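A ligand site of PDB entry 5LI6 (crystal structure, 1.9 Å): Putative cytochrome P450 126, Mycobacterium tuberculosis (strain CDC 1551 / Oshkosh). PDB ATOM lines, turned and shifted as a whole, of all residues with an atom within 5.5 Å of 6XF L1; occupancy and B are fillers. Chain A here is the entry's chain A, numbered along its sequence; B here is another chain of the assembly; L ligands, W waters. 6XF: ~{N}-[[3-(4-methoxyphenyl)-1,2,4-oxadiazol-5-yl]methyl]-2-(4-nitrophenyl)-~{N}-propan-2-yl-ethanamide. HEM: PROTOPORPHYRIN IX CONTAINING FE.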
ATOM      1  N   THR A  83     -12.903  29.365  27.147  1.00  0.00           N
ATOM      2  CA  THR A  83     -12.202  30.596  26.912  1.00  0.00           C
ATOM      3  C   THR A  83     -11.248  30.487  25.739  1.00  0.00           C
ATOM      4  O   THR A  83     -10.414  31.407  25.556  1.00  0.00           O
ATOM      5  CB  THR A  83     -11.437  31.063  28.202  1.00  0.00           C
ATOM      6  OG1 THR A  83     -10.472  30.050  28.588  1.00  0.00           O
ATOM      7  CG2 THR A  83     -12.441  31.232  29.350  1.00  0.00           C
ATOM      8  N   VAL A  84     -11.341  29.393  24.955  1.00  0.00           N
ATOM      9  CA  VAL A  84     -10.674  29.344  23.668  1.00  0.00           C
ATOM     10  C   VAL A  84     -11.697  29.241  22.558  1.00  0.00           C
ATOM     11  O   VAL A  84     -12.884  29.060  22.858  1.00  0.00           O
ATOM     12  CB  VAL A  84      -9.573  28.242  23.605  1.00  0.00           C
ATOM     13  CG1 VAL A  84      -8.489  28.458  24.738  1.00  0.00           C
ATOM     14  CG2 VAL A  84     -10.170  26.830  23.616  1.00  0.00           C
ATOM     15  N   LEU A  88     -15.202  23.618  24.383  1.00  0.00           N
ATOM     16  CA  LEU A  88     -14.586  22.542  25.104  1.00  0.00           C
ATOM     17  C   LEU A  88     -15.436  22.161  26.329  1.00  0.00           C
ATOM     18  O   LEU A  88     -15.868  23.024  27.052  1.00  0.00           O
ATOM     19  CB  LEU A  88     -13.163  22.890  25.573  1.00  0.00           C
ATOM     20  CG  LEU A  88     -12.147  23.250  24.487  1.00  0.00           C
ATOM     21  CD1 LEU A  88     -10.854  23.593  25.130  1.00  0.00           C
ATOM     22  CD2 LEU A  88     -11.983  22.122  23.440  1.00  0.00           C
ATOM     23  N   VAL A  90     -14.448  20.925  28.975  1.00  0.00           N
ATOM     24  CA  VAL A  90     -13.725  21.404  30.198  1.00  0.00           C
ATOM     25  C   VAL A  90     -14.247  22.732  30.759  1.00  0.00           C
ATOM     26  O   VAL A  90     -13.880  23.134  31.884  1.00  0.00           O
ATOM     27  CB  VAL A  90     -12.189  21.467  29.981  1.00  0.00           C
ATOM     28  CG1 VAL A  90     -11.653  20.136  29.422  1.00  0.00           C
ATOM     29  CG2 VAL A  90     -11.786  22.620  29.084  1.00  0.00           C
ATOM     30  N   VAL A  94     -12.423  23.930  35.044  1.00  0.00           N
ATOM     31  CA  VAL A  94     -11.133  24.489  35.395  1.00  0.00           C
ATOM     32  C   VAL A  94     -11.307  25.993  35.626  1.00  0.00           C
ATOM     33  O   VAL A  94     -12.143  26.656  35.015  1.00  0.00           O
ATOM     34  CB  VAL A  94     -10.092  24.161  34.275  1.00  0.00           C
ATOM     35  CG1 VAL A  94     -10.459  24.828  32.952  1.00  0.00           C
ATOM     36  CG2 VAL A  94      -8.744  24.594  34.726  1.00  0.00           C
ATOM     37  N   ASN A  96     -10.084  28.983  35.092  1.00  0.00           N
ATOM     38  CA  ASN A  96     -10.108  30.021  34.083  1.00  0.00           C
ATOM     39  C   ASN A  96     -11.406  29.923  33.223  1.00  0.00           C
ATOM     40  O   ASN A  96     -11.796  30.910  32.610  1.00  0.00           O
ATOM     41  CB  ASN A  96      -8.793  30.054  33.240  1.00  0.00           C
ATOM     42  CG  ASN A  96      -8.508  28.765  32.467  1.00  0.00           C
ATOM     43  OD1 ASN A  96      -8.585  27.646  33.007  1.00  0.00           O
ATOM     44  ND2 ASN A  96      -8.164  28.892  31.202  1.00  0.00           N
ATOM     45  N   MET A  97     -12.026  28.740  33.212  1.00  0.00           N
ATOM     46  CA  MET A  97     -13.257  28.489  32.494  1.00  0.00           C
ATOM     47  C   MET A  97     -14.452  28.288  33.454  1.00  0.00           C
ATOM     48  O   MET A  97     -15.344  27.494  33.160  1.00  0.00           O
ATOM     49  CB  MET A  97     -13.130  27.327  31.532  1.00  0.00           C
ATOM     50  CG  MET A  97     -11.907  27.526  30.613  1.00  0.00           C
ATOM     51  SD  MET A  97     -12.120  26.517  29.138  1.00  0.00           S
ATOM     52  CE  MET A  97     -10.424  26.481  28.526  1.00  0.00           C
ATOM     53  N   LEU A 245      -6.949  18.355  35.572  1.00  0.00           N
ATOM     54  CA  LEU A 245      -6.999  19.496  34.610  1.00  0.00           C
ATOM     55  C   LEU A 245      -6.306  20.782  35.146  1.00  0.00           C
ATOM     56  O   LEU A 245      -5.676  21.532  34.404  1.00  0.00           O
ATOM     57  CB  LEU A 245      -8.433  19.856  34.276  1.00  0.00           C
ATOM     58  CG  LEU A 245      -9.373  18.912  33.547  1.00  0.00           C
ATOM     59  CD1 LEU A 245     -10.818  19.535  33.536  1.00  0.00           C
ATOM     60  CD2 LEU A 245      -8.919  18.561  32.175  1.00  0.00           C
ATOM     61  N   LEU A 249      -3.004  22.460  33.453  1.00  0.00           N
ATOM     62  CA  LEU A 249      -3.114  23.886  33.091  1.00  0.00           C
ATOM     63  C   LEU A 249      -1.913  24.708  33.598  1.00  0.00           C
ATOM     64  O   LEU A 249      -1.261  25.429  32.827  1.00  0.00           O
ATOM     65  CB  LEU A 249      -4.433  24.494  33.660  1.00  0.00           C
ATOM     66  CG  LEU A 249      -4.605  26.022  33.454  1.00  0.00           C
ATOM     67  CD1 LEU A 249      -4.954  26.257  31.979  1.00  0.00           C
ATOM     68  CD2 LEU A 249      -5.576  26.746  34.469  1.00  0.00           C
ATOM     69  N   LEU A 250      -1.601  24.584  34.884  1.00  0.00           N
ATOM     70  CA  LEU A 250      -0.468  25.364  35.437  1.00  0.00           C
ATOM     71  C   LEU A 250       0.793  24.976  34.783  1.00  0.00           C
ATOM     72  O   LEU A 250       1.673  25.751  34.404  1.00  0.00           O
ATOM     73  CB  LEU A 250      -0.327  25.074  36.944  1.00  0.00           C
ATOM     74  CG  LEU A 250      -0.930  26.163  37.794  1.00  0.00           C
ATOM     75  CD1 LEU A 250      -2.394  26.180  37.563  1.00  0.00           C
ATOM     76  CD2 LEU A 250      -0.597  25.818  39.275  1.00  0.00           C
ATOM     77  N   SER A 252       1.291  23.462  31.704  1.00  0.00           N
ATOM     78  CA  SER A 252       1.413  23.852  30.227  1.00  0.00           C
ATOM     79  C   SER A 252       0.794  25.229  29.715  1.00  0.00           C
ATOM     80  O   SER A 252       0.599  25.539  28.392  1.00  0.00           O
ATOM     81  CB  SER A 252       0.747  22.800  29.342  1.00  0.00           C
ATOM     82  OG  SER A 252      -0.632  23.122  29.247  1.00  0.00           O
ATOM     83  N   ALA A 253       0.388  26.020  30.684  1.00  0.00           N
ATOM     84  CA  ALA A 253       0.043  27.383  30.408  1.00  0.00           C
ATOM     85  C   ALA A 253       1.005  28.270  31.228  1.00  0.00           C
ATOM     86  O   ALA A 253       1.642  29.120  30.668  1.00  0.00           O
ATOM     87  CB  ALA A 253      -1.407  27.649  30.701  1.00  0.00           C
ATOM     88  N   GLY A 254       1.099  28.043  32.551  1.00  0.00           N
ATOM     89  CA  GLY A 254       1.977  28.870  33.402  1.00  0.00           C
ATOM     90  C   GLY A 254       3.451  28.809  32.968  1.00  0.00           C
ATOM     91  O   GLY A 254       4.157  29.825  32.938  1.00  0.00           O
ATOM     92  N   ALA A 255       3.941  27.609  32.665  1.00  0.00           N
ATOM     93  CA  ALA A 255       5.344  27.432  32.250  1.00  0.00           C
ATOM     94  C   ALA A 255       5.539  28.022  30.865  1.00  0.00           C
ATOM     95  O   ALA A 255       6.425  28.815  30.665  1.00  0.00           O
ATOM     96  CB  ALA A 255       5.819  25.907  32.333  1.00  0.00           C
ATOM     97  N   THR A 257       3.644  30.281  28.985  1.00  0.00           N
ATOM     98  CA  THR A 257       3.538  31.730  28.852  1.00  0.00           C
ATOM     99  C   THR A 257       4.780  32.454  29.388  1.00  0.00           C
ATOM    100  O   THR A 257       5.284  33.403  28.813  1.00  0.00           O
ATOM    101  CB  THR A 257       2.291  32.298  29.577  1.00  0.00           C
ATOM    102  OG1 THR A 257       2.246  31.813  30.899  1.00  0.00           O
ATOM    103  CG2 THR A 257       0.944  31.945  28.825  1.00  0.00           C
ATOM    104  N   PRO A 299       2.167  36.977  25.497  1.00  0.00           N
ATOM    105  CA  PRO A 299       2.261  35.526  25.310  1.00  0.00           C
ATOM    106  C   PRO A 299       0.937  34.863  25.259  1.00  0.00           C
ATOM    107  O   PRO A 299       0.827  33.775  24.682  1.00  0.00           O
ATOM    108  CB  PRO A 299       2.990  35.060  26.563  1.00  0.00           C
ATOM    109  CG  PRO A 299       3.809  36.268  27.009  1.00  0.00           C
ATOM    110  CD  PRO A 299       2.847  37.406  26.736  1.00  0.00           C
ATOM    111  N   SER A 300      -0.112  35.523  25.815  1.00  0.00           N
ATOM    112  CA  SER A 300      -1.457  35.006  25.638  1.00  0.00           C
ATOM    113  C   SER A 300      -2.224  36.078  24.863  1.00  0.00           C
ATOM    114  O   SER A 300      -2.873  36.905  25.490  1.00  0.00           O
ATOM    115  CB  SER A 300      -2.089  34.781  27.035  1.00  0.00           C
ATOM    116  OG  SER A 300      -3.473  34.374  26.951  1.00  0.00           O
ATOM    117  N   SER A 302      -4.821  36.226  22.709  1.00  0.00           N
ATOM    118  CA  SER A 302      -6.263  36.009  22.356  1.00  0.00           C
ATOM    119  C   SER A 302      -7.039  35.420  23.522  1.00  0.00           C
ATOM    120  O   SER A 302      -6.522  34.691  24.387  1.00  0.00           O
ATOM    121  CB  SER A 302      -6.371  35.137  21.118  1.00  0.00           C
ATOM    122  OG  SER A 302      -5.866  33.830  21.384  1.00  0.00           O
ATOM    123  N   LYS A 303      -8.296  35.744  23.600  1.00  0.00           N
ATOM    124  CA  LYS A 303      -9.126  35.133  24.644  1.00  0.00           C
ATOM    125  C   LYS A 303     -10.566  35.021  24.124  1.00  0.00           C
ATOM    126  O   LYS A 303     -11.060  35.941  23.446  1.00  0.00           O
ATOM    127  CB  LYS A 303      -9.039  36.058  25.849  1.00  0.00           C
ATOM    128  CG  LYS A 303      -8.803  35.476  27.218  1.00  0.00           C
ATOM    129  CD  LYS A 303      -7.731  34.390  27.430  1.00  0.00           C
ATOM    130  CE  LYS A 303      -6.381  35.014  27.839  1.00  0.00           C
ATOM    131  NZ  LYS A 303      -5.808  36.044  26.916  1.00  0.00           N
ATOM    132  N   ARG A 400      -3.307  31.060  19.979  1.00  0.00           N
ATOM    133  CA  ARG A 400      -3.608  30.982  21.410  1.00  0.00           C
ATOM    134  C   ARG A 400      -2.367  31.409  22.250  1.00  0.00           C
ATOM    135  O   ARG A 400      -2.495  31.977  23.334  1.00  0.00           O
ATOM    136  CB  ARG A 400      -4.134  29.609  21.739  1.00  0.00           C
ATOM    137  CG  ARG A 400      -4.348  29.305  23.246  1.00  0.00           C
ATOM    138  CD  ARG A 400      -4.522  27.779  23.533  1.00  0.00           C
ATOM    139  NE  ARG A 400      -5.622  27.313  22.715  1.00  0.00           N
ATOM    140  CZ  ARG A 400      -5.926  26.024  22.555  1.00  0.00           C
ATOM    141  NH1 ARG A 400      -5.209  25.101  23.177  1.00  0.00           N
ATOM    142  NH2 ARG A 400      -6.933  25.678  21.800  1.00  0.00           N
ATOM    143  N   HIS A 401      -1.181  31.073  21.735  1.00  0.00           N
ATOM    144  CA  HIS A 401       0.093  31.475  22.308  1.00  0.00           C
ATOM    145  C   HIS A 401       0.849  32.302  21.300  1.00  0.00           C
ATOM    146  O   HIS A 401       0.825  31.935  20.147  1.00  0.00           O
ATOM    147  CB  HIS A 401       0.982  30.248  22.568  1.00  0.00           C
ATOM    148  CG  HIS A 401       0.490  29.341  23.646  1.00  0.00           C
ATOM    149  ND1 HIS A 401       0.877  29.489  24.941  1.00  0.00           N
ATOM    150  CD2 HIS A 401      -0.299  28.231  23.596  1.00  0.00           C
ATOM    151  CE1 HIS A 401       0.330  28.526  25.678  1.00  0.00           C
ATOM    152  NE2 HIS A 401      -0.402  27.756  24.886  1.00  0.00           N
ATOM    153  N   TYR B 203      -8.773  14.883  20.488  1.00  0.00           N
ATOM    154  CA  TYR B 203      -9.774  15.415  21.381  1.00  0.00           C
ATOM    155  C   TYR B 203     -10.602  16.433  20.561  1.00  0.00           C
ATOM    156  O   TYR B 203     -11.859  16.373  20.513  1.00  0.00           O
ATOM    157  CB  TYR B 203      -9.106  16.060  22.601  1.00  0.00           C
ATOM    158  CG  TYR B 203     -10.027  16.663  23.649  1.00  0.00           C
ATOM    159  CD1 TYR B 203     -10.951  15.896  24.302  1.00  0.00           C
ATOM    160  CD2 TYR B 203      -9.943  18.008  23.976  1.00  0.00           C
ATOM    161  CE1 TYR B 203     -11.800  16.432  25.249  1.00  0.00           C
ATOM    162  CE2 TYR B 203     -10.784  18.564  24.943  1.00  0.00           C
ATOM    163  CZ  TYR B 203     -11.733  17.778  25.551  1.00  0.00           C
ATOM    164  OH  TYR B 203     -12.566  18.320  26.500  1.00  0.00           O
HETATM  165  CAA 6XF L   1      -8.698  20.947  27.579  1.00  0.00           C
HETATM  166  OAS 6XF L   1      -7.932  21.591  26.520  1.00  0.00           O
HETATM  167  CAW 6XF L   1      -7.616  22.900  26.977  1.00  0.00           C
HETATM  168  CAJ 6XF L   1      -7.648  23.339  28.305  1.00  0.00           C
HETATM  169  CAL 6XF L   1      -7.284  24.673  28.621  1.00  0.00           C
HETATM  170  CAI 6XF L   1      -7.249  23.817  26.021  1.00  0.00           C
HETATM  171  CAK 6XF L   1      -6.907  25.115  26.339  1.00  0.00           C
HETATM  172  CAX 6XF L   1      -6.931  25.558  27.625  1.00  0.00           C
HETATM  173  CBA 6XF L   1      -6.590  26.908  27.848  1.00  0.00           C
HETATM  174  NAR 6XF L   1      -5.953  27.756  26.984  1.00  0.00           N
HETATM  175  NAQ 6XF L   1      -6.808  27.541  28.973  1.00  0.00           N
HETATM  176  OAT 6XF L   1      -6.352  28.887  28.825  1.00  0.00           O
HETATM  177  CAZ 6XF L   1      -5.835  28.948  27.584  1.00  0.00           C
HETATM  178  CAP 6XF L   1      -5.177  30.179  27.073  1.00  0.00           C
HETATM  179  NBC 6XF L   1      -4.200  30.767  28.005  1.00  0.00           N
HETATM  180  CBB 6XF L   1      -2.800  30.368  27.911  1.00  0.00           C
HETATM  181  CAC 6XF L   1      -2.679  28.801  27.847  1.00  0.00           C
HETATM  182  CAB 6XF L   1      -2.130  31.124  26.740  1.00  0.00           C
HETATM  183  CAU 6XF L   1      -4.678  31.637  28.893  1.00  0.00           C
HETATM  184  OAD 6XF L   1      -5.886  31.953  28.900  1.00  0.00           O
HETATM  185  CAO 6XF L   1      -3.662  32.326  29.801  1.00  0.00           C
HETATM  186  CAV 6XF L   1      -3.356  31.490  30.965  1.00  0.00           C
HETATM  187  CAG 6XF L   1      -2.037  31.495  31.393  1.00  0.00           C
HETATM  188  CAM 6XF L   1      -1.668  30.743  32.505  1.00  0.00           C
HETATM  189  CAY 6XF L   1      -2.593  29.996  33.147  1.00  0.00           C
HETATM  190  NBD 6XF L   1      -2.197  29.217  34.166  1.00  0.00           N
HETATM  191  OAF 6XF L   1      -0.956  28.937  34.368  1.00  0.00           O
HETATM  192  OAE 6XF L   1      -3.035  28.527  34.944  1.00  0.00           O
HETATM  193  CAN 6XF L   1      -3.925  29.962  32.714  1.00  0.00           C
HETATM  194  CAH 6XF L   1      -4.317  30.710  31.606  1.00  0.00           C
HETATM  195  CHA HEM L   2      -4.942  33.778  34.049  1.00  0.00           C
HETATM  196  CHB HEM L   2      -1.485  35.488  31.254  1.00  0.00           C
HETATM  197  CHC HEM L   2       1.863  33.360  33.950  1.00  0.00           C
HETATM  198  CHD HEM L   2      -1.577  31.332  36.598  1.00  0.00           C
HETATM  199  C1A HEM L   2      -4.307  34.492  33.095  1.00  0.00           C
HETATM  200  C2A HEM L   2      -4.968  35.309  32.078  1.00  0.00           C
HETATM  201  C3A HEM L   2      -3.988  35.781  31.289  1.00  0.00           C
HETATM  202  C4A HEM L   2      -2.725  35.229  31.781  1.00  0.00           C
HETATM  203  CMA HEM L   2      -4.104  36.745  30.073  1.00  0.00           C
HETATM  204  CAA HEM L   2      -6.488  35.579  31.982  1.00  0.00           C
HETATM  205  CBA HEM L   2      -7.308  34.430  31.404  1.00  0.00           C
HETATM  206  CGA HEM L   2      -8.716  34.847  30.994  1.00  0.00           C
HETATM  207  O1A HEM L   2      -9.131  36.056  31.149  1.00  0.00           O
HETATM  208  O2A HEM L   2      -9.451  33.906  30.611  1.00  0.00           O
HETATM  209  C1B HEM L   2      -0.278  35.033  31.680  1.00  0.00           C
HETATM  210  C2B HEM L   2       0.989  35.447  31.128  1.00  0.00           C
HETATM  211  C3B HEM L   2       1.919  34.866  31.909  1.00  0.00           C
HETATM  212  C4B HEM L   2       1.259  34.138  32.977  1.00  0.00           C
HETATM  213  CMB HEM L   2       1.272  36.404  29.892  1.00  0.00           C
HETATM  214  CAB HEM L   2       3.417  34.932  31.743  1.00  0.00           C
HETATM  215  CBB HEM L   2       4.061  35.967  31.294  1.00  0.00           C
HETATM  216  C1C HEM L   2       1.249  32.652  34.913  1.00  0.00           C
HETATM  217  C2C HEM L   2       1.904  31.824  35.909  1.00  0.00           C
HETATM  218  C3C HEM L   2       0.951  31.270  36.664  1.00  0.00           C
HETATM  219  C4C HEM L   2      -0.340  31.680  36.137  1.00  0.00           C
HETATM  220  CMC HEM L   2       3.423  31.738  36.087  1.00  0.00           C
HETATM  221  CAC HEM L   2       1.145  30.349  37.865  1.00  0.00           C
HETATM  222  CBC HEM L   2       0.576  30.692  39.024  1.00  0.00           C
HETATM  223  C1D HEM L   2      -2.794  31.758  36.081  1.00  0.00           C
HETATM  224  C2D HEM L   2      -4.053  31.271  36.550  1.00  0.00           C
HETATM  225  C3D HEM L   2      -5.063  32.051  35.821  1.00  0.00           C
HETATM  226  C4D HEM L   2      -4.334  32.884  34.916  1.00  0.00           C
HETATM  227  CMD HEM L   2      -4.370  30.212  37.636  1.00  0.00           C
HETATM  228  CAD HEM L   2      -6.602  31.867  35.962  1.00  0.00           C
HETATM  229  CBD HEM L   2      -7.146  32.790  37.019  1.00  0.00           C
HETATM  230  CGD HEM L   2      -8.657  32.814  37.040  1.00  0.00           C
HETATM  231  O1D HEM L   2      -9.237  33.239  38.077  1.00  0.00           O
HETATM  232  O2D HEM L   2      -9.300  32.404  36.044  1.00  0.00           O
HETATM  233  NA  HEM L   2      -2.963  34.492  32.862  1.00  0.00           N
HETATM  234  NB  HEM L   2      -0.111  34.267  32.832  1.00  0.00           N
HETATM  235  NC  HEM L   2      -0.125  32.565  35.139  1.00  0.00           N
HETATM  236  ND  HEM L   2      -2.978  32.802  35.182  1.00  0.00           N
HETATM  237 FE   HEM L   2      -1.537  33.623  34.079  1.00  0.00          FE
HETATM  238  O   HOH W   1      -8.576  31.394  29.903  1.00  0.00           O
HETATM  239  O   HOH W   2      -4.197  33.103  24.966  1.00  0.00           O
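Water W1 lies within hydrogen-bond range of OG1 of Thr 83 (2.7 Å), O2A of HEM L2 (2.8 Å), ND2 of Asn 96 (2.8 Å) and OAD of 6XF L1 (2.9 Å).
Water W2 lies within hydrogen-bond range of OG of Ser 300 (2.5 Å), O of Arg 400 (2.6 Å) and O of Ser 302 (2.9 Å).
Residues that only touch 6XF L1: Leu 249, Lys 303, Ala 253, Val 84, Ser 300, Arg 400, Leu 250, Val 90, Met 97, His 401, Leu 88 and Thr 257.
Hydrophobic or aromatic side chains that line 6XF L1: Val 84, Leu 88, Val 90, Met 97, Leu 249, Leu 250, Ala 253 and His 401.
The nearest printed residue that does not touch 6XF L1 is Tyr 203 of chain B (4.1 Å).
The backbone carbonyl oxygen of Gly 254 lies within hydrogen-bond range of the side-chain hydroxyl of Thr 257.
OG of Ser 300 lies within hydrogen-bond range of NZ of Lys 303, at 2.9 Å.
The backbone carbonyl oxygen of Ala 253 lies within hydrogen-bond range of the side-chain hydroxyl of Thr 257 (2.8 Å).
O of Leu 250 is in hydrogen-bond range of N of Ala 255, 3.4 Å away.
SD of Met 97 lies within hydrogen-bond range of N of Thr 83, 3.6 Å away.
N of Gly 254 lies within hydrogen-bond range of OAF of 6XF L1, at 2.9 Å.
A nitrogen (NAQ) of 6XF L1 lies within hydrogen-bond range of the side-chain amide nitrogen (ND2) of Asn 96 (2.9 Å).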
